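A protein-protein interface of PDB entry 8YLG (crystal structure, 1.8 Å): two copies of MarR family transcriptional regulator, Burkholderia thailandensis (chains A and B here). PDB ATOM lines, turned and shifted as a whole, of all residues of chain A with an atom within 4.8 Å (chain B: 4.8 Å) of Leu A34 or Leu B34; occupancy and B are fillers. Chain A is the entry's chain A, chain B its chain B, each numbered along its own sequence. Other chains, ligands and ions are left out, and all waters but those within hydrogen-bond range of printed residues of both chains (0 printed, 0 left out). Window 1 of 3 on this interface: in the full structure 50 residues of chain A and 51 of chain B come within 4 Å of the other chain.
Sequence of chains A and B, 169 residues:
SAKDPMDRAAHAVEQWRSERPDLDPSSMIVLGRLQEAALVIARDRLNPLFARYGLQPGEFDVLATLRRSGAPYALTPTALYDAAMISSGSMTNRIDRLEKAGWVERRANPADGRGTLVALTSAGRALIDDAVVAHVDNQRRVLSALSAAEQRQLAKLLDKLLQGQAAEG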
ATOM      1  N   VAL A  30      -5.295 -33.544  16.361  1.00  0.00           N
ATOM      2  CA  VAL A  30      -6.052 -32.867  15.309  1.00  0.00           C
ATOM      3  C   VAL A  30      -6.873 -31.722  15.892  1.00  0.00           C
ATOM      4  O   VAL A  30      -6.849 -30.604  15.371  1.00  0.00           O
ATOM      5  CB  VAL A  30      -6.921 -33.870  14.525  1.00  0.00           C
ATOM      6  CG1 VAL A  30      -7.778 -34.645  15.446  1.00  0.00           C
ATOM      7  CG2 VAL A  30      -7.807 -33.130  13.539  1.00  0.00           C
ATOM      8  N   LEU A  31      -7.584 -31.963  17.004  1.00  0.00           N
ATOM      9  CA  LEU A  31      -8.451 -30.908  17.526  1.00  0.00           C
ATOM     10  C   LEU A  31      -7.650 -29.785  18.167  1.00  0.00           C
ATOM     11  O   LEU A  31      -8.080 -28.624  18.128  1.00  0.00           O
ATOM     12  CB  LEU A  31      -9.461 -31.472  18.522  1.00  0.00           C
ATOM     13  CG  LEU A  31     -10.584 -32.260  17.848  1.00  0.00           C
ATOM     14  CD1 LEU A  31     -11.537 -32.748  18.914  1.00  0.00           C
ATOM     15  CD2 LEU A  31     -11.336 -31.443  16.772  1.00  0.00           C
ATOM     16  N   GLY A  32      -6.520 -30.113  18.795  1.00  0.00           N
ATOM     17  CA  GLY A  32      -5.639 -29.070  19.304  1.00  0.00           C
ATOM     18  C   GLY A  32      -5.063 -28.201  18.199  1.00  0.00           C
ATOM     19  O   GLY A  32      -4.956 -26.977  18.346  1.00  0.00           O
ATOM     20  N   ARG A  33      -4.671 -28.819  17.082  1.00  0.00           N
ATOM     21  CA  ARG A  33      -4.128 -28.025  15.975  1.00  0.00           C
ATOM     22  C   ARG A  33      -5.221 -27.193  15.309  1.00  0.00           C
ATOM     23  O   ARG A  33      -4.961 -26.075  14.846  1.00  0.00           O
ATOM     24  CB  ARG A  33      -3.441 -28.931  14.956  1.00  0.00           C
ATOM     25  CG  ARG A  33      -2.120 -29.488  15.460  1.00  0.00           C
ATOM     26  CD  ARG A  33      -1.401 -30.343  14.432  1.00  0.00           C
ATOM     27  NE  ARG A  33      -0.155 -30.879  14.993  1.00  0.00           N
ATOM     28  CZ  ARG A  33       0.428 -31.997  14.578  1.00  0.00           C
ATOM     29  NH1 ARG A  33      -0.104 -32.694  13.583  1.00  0.00           N
ATOM     30  NH2 ARG A  33       1.551 -32.417  15.154  1.00  0.00           N
ATOM     31  N   LEU A  34      -6.443 -27.730  15.229  1.00  0.00           N
ATOM     32  CA  LEU A  34      -7.562 -26.956  14.684  1.00  0.00           C
ATOM     33  C   LEU A  34      -7.794 -25.697  15.507  1.00  0.00           C
ATOM     34  O   LEU A  34      -7.899 -24.590  14.965  1.00  0.00           O
ATOM     35  CB  LEU A  34      -8.837 -27.807  14.657  1.00  0.00           C
ATOM     36  CG  LEU A  34     -10.143 -27.104  14.260  1.00  0.00           C
ATOM     37  CD1 LEU A  34     -10.110 -26.751  12.828  1.00  0.00           C
ATOM     38  CD2 LEU A  34     -11.356 -27.971  14.547  1.00  0.00           C
ATOM     39  N   GLN A  35      -7.875 -25.856  16.827  1.00  0.00           N
ATOM     40  CA  GLN A  35      -8.077 -24.720  17.717  1.00  0.00           C
ATOM     41  C   GLN A  35      -6.926 -23.724  17.606  1.00  0.00           C
ATOM     42  O   GLN A  35      -7.144 -22.509  17.496  1.00  0.00           O
ATOM     43  CB  GLN A  35      -8.217 -25.237  19.154  1.00  0.00           C
ATOM     44  CG  GLN A  35      -8.396 -24.168  20.222  1.00  0.00           C
ATOM     45  CD  GLN A  35      -8.872 -24.751  21.556  1.00  0.00           C
ATOM     46  OE1 GLN A  35      -8.287 -24.487  22.610  1.00  0.00           O
ATOM     47  NE2 GLN A  35      -9.940 -25.546  21.509  1.00  0.00           N
ATOM     48  N   GLU A  36      -5.689 -24.228  17.637  1.00  0.00           N
ATOM     49  CA  GLU A  36      -4.521 -23.350  17.576  1.00  0.00           C
ATOM     50  C   GLU A  36      -4.448 -22.605  16.243  1.00  0.00           C
ATOM     51  O   GLU A  36      -4.133 -21.408  16.210  1.00  0.00           O
ATOM     52  CB  GLU A  36      -3.245 -24.159  17.805  1.00  0.00           C
ATOM     53  CG  GLU A  36      -1.995 -23.293  17.843  1.00  0.00           C
ATOM     54  CD  GLU A  36      -0.758 -24.088  18.159  1.00  0.00           C
ATOM     55  OE1 GLU A  36      -0.893 -25.177  18.773  1.00  0.00           O
ATOM     56  OE2 GLU A  36       0.337 -23.623  17.784  1.00  0.00           O
ATOM     57  N   ALA A  37      -4.715 -23.299  15.134  1.00  0.00           N
ATOM     58  CA  ALA A  37      -4.692 -22.648  13.824  1.00  0.00           C
ATOM     59  C   ALA A  37      -5.727 -21.535  13.742  1.00  0.00           C
ATOM     60  O   ALA A  37      -5.435 -20.438  13.251  1.00  0.00           O
ATOM     61  CB  ALA A  37      -4.912 -23.680  12.715  1.00  0.00           C
ATOM     62  N   ALA A  38      -6.952 -21.792  14.205  1.00  0.00           N
ATOM     63  CA  ALA A  38      -7.970 -20.742  14.144  1.00  0.00           C
ATOM     64  C   ALA A  38      -7.554 -19.529  14.968  1.00  0.00           C
ATOM     65  O   ALA A  38      -7.727 -18.377  14.539  1.00  0.00           O
ATOM     66  CB  ALA A  38      -9.325 -21.269  14.617  1.00  0.00           C
ATOM     67  N   ILE A  41      -4.210 -17.727  13.324  1.00  0.00           N
ATOM     68  CA  ILE A  41      -4.493 -17.064  12.053  1.00  0.00           C
ATOM     69  C   ILE A  41      -5.321 -15.806  12.284  1.00  0.00           C
ATOM     70  O   ILE A  41      -5.027 -14.749  11.717  1.00  0.00           O
ATOM     71  CB  ILE A  41      -5.181 -18.049  11.081  1.00  0.00           C
ATOM     72  CG1 ILE A  41      -4.180 -19.088  10.581  1.00  0.00           C
ATOM     73  CG2 ILE A  41      -5.854 -17.298   9.900  1.00  0.00           C
ATOM     74  CD1 ILE A  41      -4.814 -20.231   9.811  1.00  0.00           C
ATOM     75  N   LEU A 158     -12.464 -30.385   6.302  1.00  0.00           N
ATOM     76  CA  LEU A 158     -13.200 -29.528   7.232  1.00  0.00           C
ATOM     77  C   LEU A 158     -14.698 -29.575   6.963  1.00  0.00           C
ATOM     78  O   LEU A 158     -15.504 -29.551   7.899  1.00  0.00           O
ATOM     79  CB  LEU A 158     -12.683 -28.096   7.154  1.00  0.00           C
ATOM     80  CG  LEU A 158     -11.286 -27.930   7.749  1.00  0.00           C
ATOM     81  CD1 LEU A 158     -10.691 -26.569   7.403  1.00  0.00           C
ATOM     82  CD2 LEU A 158     -11.324 -28.156   9.254  1.00  0.00           C
ATOM     83  N   LEU A 161     -16.022 -32.760   8.430  1.00  0.00           N
ATOM     84  CA  LEU A 161     -16.098 -32.623   9.879  1.00  0.00           C
ATOM     85  C   LEU A 161     -17.283 -31.756  10.287  1.00  0.00           C
ATOM     86  O   LEU A 161     -17.975 -32.061  11.265  1.00  0.00           O
ATOM     87  CB  LEU A 161     -14.783 -32.040  10.404  1.00  0.00           C
ATOM     88  CG  LEU A 161     -14.580 -31.865  11.903  1.00  0.00           C
ATOM     89  CD1 LEU A 161     -14.566 -33.203  12.593  1.00  0.00           C
ATOM     90  CD2 LEU A 161     -13.277 -31.104  12.176  1.00  0.00           C
ATOM     91  N   VAL B  30     -11.625 -22.476   2.720  1.00  0.00           N
ATOM     92  CA  VAL B  30     -10.883 -23.227   3.730  1.00  0.00           C
ATOM     93  C   VAL B  30     -10.829 -22.456   5.049  1.00  0.00           C
ATOM     94  O   VAL B  30     -11.010 -23.036   6.127  1.00  0.00           O
ATOM     95  CB  VAL B  30      -9.483 -23.620   3.223  1.00  0.00           C
ATOM     96  CG1 VAL B  30      -8.680 -22.423   2.836  1.00  0.00           C
ATOM     97  CG2 VAL B  30      -8.770 -24.468   4.274  1.00  0.00           C
ATOM     98  N   LEU B  31     -10.569 -21.147   5.000  1.00  0.00           N
ATOM     99  CA  LEU B  31     -10.415 -20.401   6.250  1.00  0.00           C
ATOM    100  C   LEU B  31     -11.756 -20.186   6.949  1.00  0.00           C
ATOM    101  O   LEU B  31     -11.825 -20.199   8.186  1.00  0.00           O
ATOM    102  CB  LEU B  31      -9.716 -19.067   5.987  1.00  0.00           C
ATOM    103  CG  LEU B  31      -8.211 -19.234   5.764  1.00  0.00           C
ATOM    104  CD1 LEU B  31      -7.531 -17.894   5.479  1.00  0.00           C
ATOM    105  CD2 LEU B  31      -7.583 -19.874   6.991  1.00  0.00           C
ATOM    106  N   GLY B  32     -12.827 -19.975   6.186  1.00  0.00           N
ATOM    107  CA  GLY B  32     -14.142 -19.887   6.803  1.00  0.00           C
ATOM    108  C   GLY B  32     -14.540 -21.197   7.464  1.00  0.00           C
ATOM    109  O   GLY B  32     -15.113 -21.208   8.558  1.00  0.00           O
ATOM    110  N   ARG B  33     -14.233 -22.321   6.816  1.00  0.00           N
ATOM    111  CA  ARG B  33     -14.565 -23.611   7.416  1.00  0.00           C
ATOM    112  C   ARG B  33     -13.695 -23.887   8.630  1.00  0.00           C
ATOM    113  O   ARG B  33     -14.172 -24.459   9.614  1.00  0.00           O
ATOM    114  CB  ARG B  33     -14.427 -24.742   6.400  1.00  0.00           C
ATOM    115  CG  ARG B  33     -15.540 -24.753   5.358  1.00  0.00           C
ATOM    116  CD  ARG B  33     -15.420 -25.918   4.395  1.00  0.00           C
ATOM    117  NE  ARG B  33     -16.496 -25.850   3.406  1.00  0.00           N
ATOM    118  CZ  ARG B  33     -16.429 -26.360   2.183  1.00  0.00           C
ATOM    119  NH1 ARG B  33     -15.343 -27.004   1.785  1.00  0.00           N
ATOM    120  NH2 ARG B  33     -17.451 -26.208   1.351  1.00  0.00           N
ATOM    121  N   LEU B  34     -12.423 -23.467   8.584  1.00  0.00           N
ATOM    122  CA  LEU B  34     -11.549 -23.619   9.740  1.00  0.00           C
ATOM    123  C   LEU B  34     -12.117 -22.888  10.946  1.00  0.00           C
ATOM    124  O   LEU B  34     -12.190 -23.441  12.048  1.00  0.00           O
ATOM    125  CB  LEU B  34     -10.152 -23.092   9.404  1.00  0.00           C
ATOM    126  CG  LEU B  34      -9.131 -23.027  10.544  1.00  0.00           C
ATOM    127  CD1 LEU B  34      -8.768 -24.401  10.932  1.00  0.00           C
ATOM    128  CD2 LEU B  34      -7.887 -22.265  10.131  1.00  0.00           C
ATOM    129  N   GLN B  35     -12.498 -21.623  10.754  1.00  0.00           N
ATOM    130  CA  GLN B  35     -13.066 -20.816  11.827  1.00  0.00           C
ATOM    131  C   GLN B  35     -14.394 -21.396  12.319  1.00  0.00           C
ATOM    132  O   GLN B  35     -14.639 -21.485  13.528  1.00  0.00           O
ATOM    133  CB  GLN B  35     -13.232 -19.374  11.329  1.00  0.00           C
ATOM    134  CG  GLN B  35     -13.851 -18.383  12.315  1.00  0.00           C
ATOM    135  CD  GLN B  35     -13.669 -16.928  11.864  1.00  0.00           C
ATOM    136  OE1 GLN B  35     -14.633 -16.157  11.798  1.00  0.00           O
ATOM    137  NE2 GLN B  35     -12.426 -16.548  11.560  1.00  0.00           N
ATOM    138  N   GLU B  36     -15.271 -21.790  11.392  1.00  0.00           N
ATOM    139  CA  GLU B  36     -16.560 -22.348  11.793  1.00  0.00           C
ATOM    140  C   GLU B  36     -16.390 -23.663  12.562  1.00  0.00           C
ATOM    141  O   GLU B  36     -17.063 -23.890  13.579  1.00  0.00           O
ATOM    142  CB  GLU B  36     -17.437 -22.558  10.565  1.00  0.00           C
ATOM    143  CG  GLU B  36     -18.825 -23.077  10.905  1.00  0.00           C
ATOM    144  CD  GLU B  36     -19.732 -23.189   9.692  1.00  0.00           C
ATOM    145  OE1 GLU B  36     -19.501 -22.471   8.684  1.00  0.00           O
ATOM    146  OE2 GLU B  36     -20.677 -24.006   9.747  1.00  0.00           O
ATOM    147  N   ALA B  37     -15.506 -24.547  12.088  1.00  0.00           N
ATOM    148  CA  ALA B  37     -15.302 -25.825  12.772  1.00  0.00           C
ATOM    149  C   ALA B  37     -14.790 -25.616  14.192  1.00  0.00           C
ATOM    150  O   ALA B  37     -15.257 -26.269  15.135  1.00  0.00           O
ATOM    151  CB  ALA B  37     -14.330 -26.708  11.986  1.00  0.00           C
ATOM    152  N   ALA B  38     -13.809 -24.729  14.361  1.00  0.00           N
ATOM    153  CA  ALA B  38     -13.276 -24.475  15.698  1.00  0.00           C
ATOM    154  C   ALA B  38     -14.361 -23.950  16.631  1.00  0.00           C
ATOM    155  O   ALA B  38     -14.459 -24.375  17.789  1.00  0.00           O
ATOM    156  CB  ALA B  38     -12.109 -23.481  15.622  1.00  0.00           C
ATOM    157  N   ILE B  41     -17.380 -26.788  17.239  1.00  0.00           N
ATOM    158  CA  ILE B  41     -16.962 -27.916  18.071  1.00  0.00           C
ATOM    159  C   ILE B  41     -16.778 -27.476  19.519  1.00  0.00           C
ATOM    160  O   ILE B  41     -17.185 -28.179  20.457  1.00  0.00           O
ATOM    161  CB  ILE B  41     -15.691 -28.566  17.489  1.00  0.00           C
ATOM    162  CG1 ILE B  41     -16.040 -29.301  16.189  1.00  0.00           C
ATOM    163  CG2 ILE B  41     -15.032 -29.501  18.500  1.00  0.00           C
ATOM    164  CD1 ILE B  41     -14.830 -29.779  15.395  1.00  0.00           C
ATOM    165  N   LEU B 158      -3.008 -29.452   9.029  1.00  0.00           N
ATOM    166  CA  LEU B 158      -3.046 -28.377  10.011  1.00  0.00           C
ATOM    167  C   LEU B 158      -1.650 -28.066  10.551  1.00  0.00           C
ATOM    168  O   LEU B 158      -1.339 -26.904  10.819  1.00  0.00           O
ATOM    169  CB  LEU B 158      -4.020 -28.715  11.136  1.00  0.00           C
ATOM    170  CG  LEU B 158      -5.509 -28.672  10.763  1.00  0.00           C
ATOM    171  CD1 LEU B 158      -6.379 -29.310  11.882  1.00  0.00           C
ATOM    172  CD2 LEU B 158      -5.974 -27.252  10.476  1.00  0.00           C
ATOM    173  N   LEU B 161       0.030 -25.968   7.984  1.00  0.00           N
ATOM    174  CA  LEU B 161      -0.511 -24.610   7.996  1.00  0.00           C
ATOM    175  C   LEU B 161       0.011 -23.814   9.189  1.00  0.00           C
ATOM    176  O   LEU B 161       0.365 -22.636   9.052  1.00  0.00           O
ATOM    177  CB  LEU B 161      -2.039 -24.674   7.993  1.00  0.00           C
ATOM    178  CG  LEU B 161      -2.816 -23.357   7.956  1.00  0.00           C
ATOM    179  CD1 LEU B 161      -2.542 -22.601   6.677  1.00  0.00           C
ATOM    180  CD2 LEU B 161      -4.321 -23.637   8.132  1.00  0.00           C
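Printed residues of chain B within 4 Å of Leu A34: Leu B34 and Leu B158.
Leu B34 touches just these residues of chain A: Leu A34, Ile A41 and Leu A158.
Printed residues of chain B within 4 Å of Val A30: Leu B158 (3.8 Å).
Of the printed residues of chain A, Arg B33 touches Leu A158.
Of the printed residues of chain B, Arg A33 touches Leu B158.
Of the printed residues of chain B, Ala A38 touches Ala B38.
Glu B36 touches none of the printed residues of chain A.
The nearest printed residue of chain B that does not touch Leu A34 is Ile B41 (4.01 Å).
Among the printed residues, pairs that only touch across the chains: Leu A34 with Leu B34, Ala A38 with Ala B38, Ile A41 with Leu B34, Leu A34 with Leu B158, Leu A158 with Leu B34, Val A30 with Leu B158, Leu A158 with Val B30, Leu A161 with Ile B41, Ile A41 with Leu B161, Leu A158 with Arg B33, Arg A33 with Leu B158 and Ile A41 with Leu B31.
Arg A33 touches Leu B158, and with the chains exchanged Leu A158 touches Arg B33.
Leu B34 touches its own counterpart, Leu A34.
Leu A34 touches Leu B158, and with the chains exchanged Leu A158 touches Leu B34.
Ile A41 touches Leu B161, and with the chains exchanged Leu A161 touches Ile B41.
Positions printed for both chains: 30, 31, 32, 33, 34, 35, 36, 37, 38, 41, 158 and 161.
Hydrophobic or aromatic side chains of chain B that line the printed part of chain A: Leu B31, Leu B34, Ala B38, Ile B41, Leu B158 and Leu B161.
Printed residues of chain A that touch a printed residue of chain B: Val A30, Arg A33, Leu A34, Ala A38, Ile A41, Leu A158 and Leu A161.
Hydrophobic or aromatic side chains of chain A within 4 Å of the printed part of chain B: Leu A34, Ala A38, Ile A41, Leu A158 and Leu A161.
Among the printed residues, 12 pairs touch across the chains.
Among the printed residues, no Asp or Glu carboxylate lies within 4 Å of a Lys or Arg side-chain nitrogen of the other chain.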
